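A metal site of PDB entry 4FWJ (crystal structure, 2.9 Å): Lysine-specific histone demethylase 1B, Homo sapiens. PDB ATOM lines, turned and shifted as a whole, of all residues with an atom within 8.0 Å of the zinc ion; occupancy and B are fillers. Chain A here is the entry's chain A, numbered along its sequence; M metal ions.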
ATOM      1  N   VAL A  38       9.603  29.972  -3.787  1.00  0.00           N
ATOM      2  CA  VAL A  38       9.495  28.805  -4.656  1.00  0.00           C
ATOM      3  C   VAL A  38      10.598  27.819  -4.268  1.00  0.00           C
ATOM      4  O   VAL A  38      11.691  28.241  -3.893  1.00  0.00           O
ATOM      5  CB  VAL A  38       9.613  29.226  -6.123  1.00  0.00           C
ATOM      6  CG1 VAL A  38       9.471  28.025  -7.049  1.00  0.00           C
ATOM      7  CG2 VAL A  38       8.558  30.264  -6.463  1.00  0.00           C
ATOM      8  N   CYS A  39      10.320  26.520  -4.354  1.00  0.00           N
ATOM      9  CA  CYS A  39      11.307  25.533  -3.910  1.00  0.00           C
ATOM     10  C   CYS A  39      12.334  25.202  -4.978  1.00  0.00           C
ATOM     11  O   CYS A  39      11.967  24.745  -6.055  1.00  0.00           O
ATOM     12  CB  CYS A  39      10.635  24.253  -3.454  1.00  0.00           C
ATOM     13  SG  CYS A  39      11.816  23.182  -2.629  1.00  0.00           S
ATOM     14  N   PHE A  40      13.615  25.433  -4.679  1.00  0.00           N
ATOM     15  CA  PHE A  40      14.680  25.281  -5.674  1.00  0.00           C
ATOM     16  C   PHE A  40      15.062  23.813  -5.915  1.00  0.00           C
ATOM     17  O   PHE A  40      15.569  23.476  -6.984  1.00  0.00           O
ATOM     18  CB  PHE A  40      15.921  26.113  -5.314  1.00  0.00           C
ATOM     19  CG  PHE A  40      16.693  25.611  -4.125  1.00  0.00           C
ATOM     20  CD1 PHE A  40      16.599  26.267  -2.901  1.00  0.00           C
ATOM     21  CD2 PHE A  40      17.504  24.478  -4.219  1.00  0.00           C
ATOM     22  CE1 PHE A  40      17.298  25.800  -1.801  1.00  0.00           C
ATOM     23  CE2 PHE A  40      18.200  24.002  -3.120  1.00  0.00           C
ATOM     24  CZ  PHE A  40      18.100  24.672  -1.905  1.00  0.00           C
ATOM     25  N   ALA A  41      14.851  22.963  -4.907  1.00  0.00           N
ATOM     26  CA  ALA A  41      15.077  21.534  -5.049  1.00  0.00           C
ATOM     27  C   ALA A  41      13.799  20.904  -5.557  1.00  0.00           C
ATOM     28  O   ALA A  41      12.750  21.550  -5.601  1.00  0.00           O
ATOM     29  CB  ALA A  41      15.466  20.928  -3.715  1.00  0.00           C
ATOM     30  N   SER A  42      13.852  19.653  -5.957  1.00  0.00           N
ATOM     31  CA  SER A  42      12.636  18.955  -6.269  1.00  0.00           C
ATOM     32  C   SER A  42      12.805  17.511  -5.831  1.00  0.00           C
ATOM     33  O   SER A  42      12.364  16.579  -6.503  1.00  0.00           O
ATOM     34  CB  SER A  42      12.317  19.079  -7.758  1.00  0.00           C
ATOM     35  OG  SER A  42      12.204  20.441  -8.113  1.00  0.00           O
ATOM     36  N   ALA A  43      13.444  17.365  -4.674  1.00  0.00           N
ATOM     37  CA  ALA A  43      13.851  16.065  -4.159  1.00  0.00           C
ATOM     38  C   ALA A  43      12.656  15.176  -3.808  1.00  0.00           C
ATOM     39  O   ALA A  43      12.741  13.954  -3.951  1.00  0.00           O
ATOM     40  CB  ALA A  43      14.756  16.238  -2.954  1.00  0.00           C
ATOM     41  N   SER A  44      11.557  15.796  -3.373  1.00  0.00           N
ATOM     42  CA  SER A  44      10.417  15.039  -2.873  1.00  0.00           C
ATOM     43  C   SER A  44       9.334  14.774  -3.894  1.00  0.00           C
ATOM     44  O   SER A  44       9.091  15.592  -4.793  1.00  0.00           O
ATOM     45  CB  SER A  44       9.792  15.715  -1.647  1.00  0.00           C
ATOM     46  OG  SER A  44       8.834  14.843  -1.063  1.00  0.00           O
ATOM     47  N   GLU A  45       8.693  13.619  -3.745  1.00  0.00           N
ATOM     48  CA  GLU A  45       7.535  13.223  -4.553  1.00  0.00           C
ATOM     49  C   GLU A  45       6.418  14.260  -4.401  1.00  0.00           C
ATOM     50  O   GLU A  45       5.718  14.569  -5.359  1.00  0.00           O
ATOM     51  CB  GLU A  45       7.042  11.849  -4.091  1.00  0.00           C
ATOM     52  CG  GLU A  45       6.236  11.055  -5.115  1.00  0.00           C
ATOM     53  CD  GLU A  45       7.046   9.985  -5.836  1.00  0.00           C
ATOM     54  OE1 GLU A  45       6.453   8.946  -6.196  1.00  0.00           O
ATOM     55  OE2 GLU A  45       8.270  10.175  -6.048  1.00  0.00           O
ATOM     56  N   ARG A  46       6.269  14.785  -3.175  1.00  0.00           N
ATOM     57  CA  ARG A  46       5.232  15.747  -2.828  1.00  0.00           C
ATOM     58  C   ARG A  46       5.780  17.155  -2.487  1.00  0.00           C
ATOM     59  O   ARG A  46       5.268  17.825  -1.590  1.00  0.00           O
ATOM     60  CB  ARG A  46       4.357  15.209  -1.686  1.00  0.00           C
ATOM     61  CG  ARG A  46       2.960  14.790  -2.113  1.00  0.00           C
ATOM     62  CD  ARG A  46       2.334  13.836  -1.113  1.00  0.00           C
ATOM     63  NE  ARG A  46       3.027  12.538  -1.100  1.00  0.00           N
ATOM     64  CZ  ARG A  46       2.669  11.478  -1.826  1.00  0.00           C
ATOM     65  NH1 ARG A  46       1.608  11.526  -2.617  1.00  0.00           N
ATOM     66  NH2 ARG A  46       3.379  10.356  -1.741  1.00  0.00           N
ATOM     67  N   CYS A  47       6.807  17.576  -3.213  1.00  0.00           N
ATOM     68  CA  CYS A  47       7.375  18.918  -3.070  1.00  0.00           C
ATOM     69  C   CYS A  47       6.339  20.012  -3.312  1.00  0.00           C
ATOM     70  O   CYS A  47       5.588  19.947  -4.286  1.00  0.00           O
ATOM     71  CB  CYS A  47       8.533  19.104  -4.041  1.00  0.00           C
ATOM     72  SG  CYS A  47       9.089  20.823  -4.217  1.00  0.00           S
ATOM     73  N   ALA A  48       6.281  20.997  -2.420  1.00  0.00           N
ATOM     74  CA  ALA A  48       5.390  22.143  -2.620  1.00  0.00           C
ATOM     75  C   ALA A  48       6.083  23.080  -3.589  1.00  0.00           C
ATOM     76  O   ALA A  48       7.009  23.793  -3.216  1.00  0.00           O
ATOM     77  CB  ALA A  48       5.096  22.832  -1.299  1.00  0.00           C
ATOM     78  N   LYS A  49       5.653  23.062  -4.848  1.00  0.00           N
ATOM     79  CA  LYS A  49       6.364  23.831  -5.867  1.00  0.00           C
ATOM     80  C   LYS A  49       6.238  25.338  -5.611  1.00  0.00           C
ATOM     81  O   LYS A  49       7.238  26.019  -5.340  1.00  0.00           O
ATOM     82  CB  LYS A  49       5.884  23.445  -7.273  1.00  0.00           C
ATOM     83  CG  LYS A  49       6.188  22.000  -7.656  1.00  0.00           C
ATOM     84  N   ASN A  50       4.998  25.825  -5.651  1.00  0.00           N
ATOM     85  CA  ASN A  50       4.655  27.218  -5.346  1.00  0.00           C
ATOM     86  C   ASN A  50       3.814  27.346  -4.094  1.00  0.00           C
ATOM     87  O   ASN A  50       3.696  28.437  -3.524  1.00  0.00           O
ATOM     88  CB  ASN A  50       3.845  27.826  -6.504  1.00  0.00           C
ATOM     89  CG  ASN A  50       4.705  28.163  -7.701  1.00  0.00           C
ATOM     90  OD1 ASN A  50       5.371  27.290  -8.263  1.00  0.00           O
ATOM     91  ND2 ASN A  50       4.677  29.429  -8.114  1.00  0.00           N
ATOM     92  N   THR A  53       4.170  24.675   1.980  1.00  0.00           N
ATOM     93  CA  THR A  53       4.870  23.740   2.843  1.00  0.00           C
ATOM     94  C   THR A  53       4.454  24.129   4.254  1.00  0.00           C
ATOM     95  O   THR A  53       3.864  25.196   4.440  1.00  0.00           O
ATOM     96  CB  THR A  53       6.404  23.879   2.717  1.00  0.00           C
ATOM     97  N   TRP A  56       8.876  27.014   5.194  1.00  0.00           N
ATOM     98  CA  TRP A  56       9.795  27.401   4.117  1.00  0.00           C
ATOM     99  C   TRP A  56      11.152  27.730   4.683  1.00  0.00           C
ATOM    100  O   TRP A  56      11.346  28.774   5.299  1.00  0.00           O
ATOM    101  CB  TRP A  56       9.282  28.638   3.389  1.00  0.00           C
ATOM    102  CG  TRP A  56       8.304  28.402   2.274  1.00  0.00           C
ATOM    103  CD1 TRP A  56       7.010  28.916   2.165  1.00  0.00           C
ATOM    104  CD2 TRP A  56       8.509  27.636   1.042  1.00  0.00           C
ATOM    105  NE1 TRP A  56       6.417  28.506   0.994  1.00  0.00           N
ATOM    106  CE2 TRP A  56       7.253  27.734   0.279  1.00  0.00           C
ATOM    107  CE3 TRP A  56       9.553  26.886   0.518  1.00  0.00           C
ATOM    108  CZ2 TRP A  56       7.085  27.114  -0.951  1.00  0.00           C
ATOM    109  CZ3 TRP A  56       9.373  26.261  -0.722  1.00  0.00           C
ATOM    110  CH2 TRP A  56       8.163  26.369  -1.432  1.00  0.00           C
ATOM    111  N   HIS A  64      14.896  29.387  -1.505  1.00  0.00           N
ATOM    112  CA  HIS A  64      14.107  28.698  -0.479  1.00  0.00           C
ATOM    113  C   HIS A  64      13.836  27.266  -0.863  1.00  0.00           C
ATOM    114  O   HIS A  64      13.765  26.936  -2.044  1.00  0.00           O
ATOM    115  CB  HIS A  64      12.764  29.409  -0.274  1.00  0.00           C
ATOM    116  CG  HIS A  64      12.910  30.845   0.155  1.00  0.00           C
ATOM    117  ND1 HIS A  64      13.198  31.831  -0.713  1.00  0.00           N
ATOM    118  CD2 HIS A  64      12.796  31.440   1.411  1.00  0.00           C
ATOM    119  CE1 HIS A  64      13.277  33.003  -0.046  1.00  0.00           C
ATOM    120  NE2 HIS A  64      13.030  32.765   1.247  1.00  0.00           N
ATOM    121  N   PHE A  65      13.702  26.391   0.136  1.00  0.00           N
ATOM    122  CA  PHE A  65      13.213  25.035  -0.106  1.00  0.00           C
ATOM    123  C   PHE A  65      12.154  24.608   0.911  1.00  0.00           C
ATOM    124  O   PHE A  65      12.095  25.152   2.012  1.00  0.00           O
ATOM    125  CB  PHE A  65      14.358  24.016  -0.214  1.00  0.00           C
ATOM    126  CG  PHE A  65      15.164  23.865   1.039  1.00  0.00           C
ATOM    127  CD1 PHE A  65      16.247  24.699   1.302  1.00  0.00           C
ATOM    128  CD2 PHE A  65      14.868  22.855   1.945  1.00  0.00           C
ATOM    129  CE1 PHE A  65      16.990  24.551   2.462  1.00  0.00           C
ATOM    130  CE2 PHE A  65      15.608  22.697   3.104  1.00  0.00           C
ATOM    131  CZ  PHE A  65      16.675  23.548   3.358  1.00  0.00           C
ATOM    132  N   CYS A  66      11.297  23.663   0.512  1.00  0.00           N
ATOM    133  CA  CYS A  66      10.120  23.265   1.286  1.00  0.00           C
ATOM    134  C   CYS A  66      10.423  22.186   2.317  1.00  0.00           C
ATOM    135  O   CYS A  66      11.431  21.483   2.252  1.00  0.00           O
ATOM    136  CB  CYS A  66       9.039  22.786   0.340  1.00  0.00           C
ATOM    137  SG  CYS A  66       9.387  21.187  -0.433  1.00  0.00           S
ATOM    138  N   ASN A  67       9.509  22.037   3.272  1.00  0.00           N
ATOM    139  CA  ASN A  67       9.653  21.048   4.348  1.00  0.00           C
ATOM    140  C   ASN A  67       9.548  19.609   3.839  1.00  0.00           C
ATOM    141  O   ASN A  67      10.035  18.668   4.481  1.00  0.00           O
ATOM    142  CB  ASN A  67       8.619  21.325   5.440  1.00  0.00           C
ATOM    143  CG  ASN A  67       8.843  20.479   6.678  1.00  0.00           C
ATOM    144  OD1 ASN A  67       8.078  19.551   6.960  1.00  0.00           O
ATOM    145  ND2 ASN A  67       9.901  20.799   7.433  1.00  0.00           N
ATOM    146  N   GLU A  68       8.927  19.429   2.685  1.00  0.00           N
ATOM    147  CA  GLU A  68       8.852  18.112   2.061  1.00  0.00           C
ATOM    148  C   GLU A  68      10.228  17.719   1.533  1.00  0.00           C
ATOM    149  O   GLU A  68      10.597  16.558   1.569  1.00  0.00           O
ATOM    150  CB  GLU A  68       7.813  18.101   0.931  1.00  0.00           C
ATOM    151  CG  GLU A  68       6.713  19.161   1.025  1.00  0.00           C
ATOM    152  CD  GLU A  68       5.550  18.772   1.931  1.00  0.00           C
ATOM    153  OE1 GLU A  68       4.601  19.587   2.043  1.00  0.00           O
ATOM    154  OE2 GLU A  68       5.573  17.677   2.517  1.00  0.00           O
ATOM    155  N   CYS A  69      10.988  18.696   1.054  1.00  0.00           N
ATOM    156  CA  CYS A  69      12.337  18.411   0.589  1.00  0.00           C
ATOM    157  C   CYS A  69      13.346  18.238   1.736  1.00  0.00           C
ATOM    158  O   CYS A  69      14.556  18.354   1.555  1.00  0.00           O
ATOM    159  CB  CYS A  69      12.778  19.412  -0.464  1.00  0.00           C
ATOM    160  SG  CYS A  69      11.964  19.133  -2.061  1.00  0.00           S
ATOM    161  N   PHE A  70      12.815  17.971   2.923  1.00  0.00           N
ATOM    162  CA  PHE A  70      13.471  17.157   3.950  1.00  0.00           C
ATOM    163  C   PHE A  70      13.196  15.648   3.678  1.00  0.00           C
ATOM    164  O   PHE A  70      13.008  14.835   4.591  1.00  0.00           O
ATOM    165  CB  PHE A  70      12.983  17.550   5.349  1.00  0.00           C
ATOM    166  CG  PHE A  70      13.747  18.688   5.978  1.00  0.00           C
ATOM    167  CD1 PHE A  70      14.094  19.816   5.250  1.00  0.00           C
ATOM    168  CD2 PHE A  70      14.081  18.640   7.336  1.00  0.00           C
ATOM    169  CE1 PHE A  70      14.791  20.852   5.854  1.00  0.00           C
ATOM    170  CE2 PHE A  70      14.775  19.665   7.949  1.00  0.00           C
ATOM    171  CZ  PHE A  70      15.138  20.779   7.210  1.00  0.00           C
ATOM    172  N   MET A 105      22.095  21.605   1.218  1.00  0.00           N
ATOM    173  CA  MET A 105      21.436  22.224   0.068  1.00  0.00           C
ATOM    174  C   MET A 105      22.364  23.197  -0.647  1.00  0.00           C
ATOM    175  O   MET A 105      22.430  23.212  -1.882  1.00  0.00           O
ATOM    176  CB  MET A 105      20.179  22.969   0.521  1.00  0.00           C
ATOM    177  CG  MET A 105      19.051  22.060   1.014  1.00  0.00           C
ATOM    178  SD  MET A 105      18.489  20.895  -0.236  1.00  0.00           S
ATOM    179  CE  MET A 105      17.133  20.091   0.603  1.00  0.00           C
HETATM  180 ZN    ZN M   1      10.537  21.165  -2.538  1.00  0.00          ZN
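SG of Cys 39 lies close to O of Ala 41 (3.5 Å). The backbone NH (N) of Ser 44 lies close to the side-chain sulfur (SG) of Cys 69, 3.6 Å away. The backbone NH of Glu 68 lies close to the side-chain sulfur of Cys 66 (3.6 Å). N of Cys 39 is in hydrogen-bond range of O of Lys 49 (3.3 Å). SG of Cys 69 sits close to N of Ala 43, 3.5 Å away. The backbone NH of Ala 48 lies close to the side-chain sulfur of Cys 66 (3.7 Å).
Ala 41 touches the zinc ion (O to ZN, 3.8 Å). Of the 23 residues printed, 5 come within 4 Å of the zinc ion.
The zinc ion is bound by the side-chain sulfur of Cys 47 (2.2 Å), the side-chain sulfur of Cys 39 (2.4 Å), the side-chain sulfur of Cys 66 (2.4 Å) and the side-chain sulfur of Cys 69 (2.5 Å). The zinc ion has four donor atoms within binding distance.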
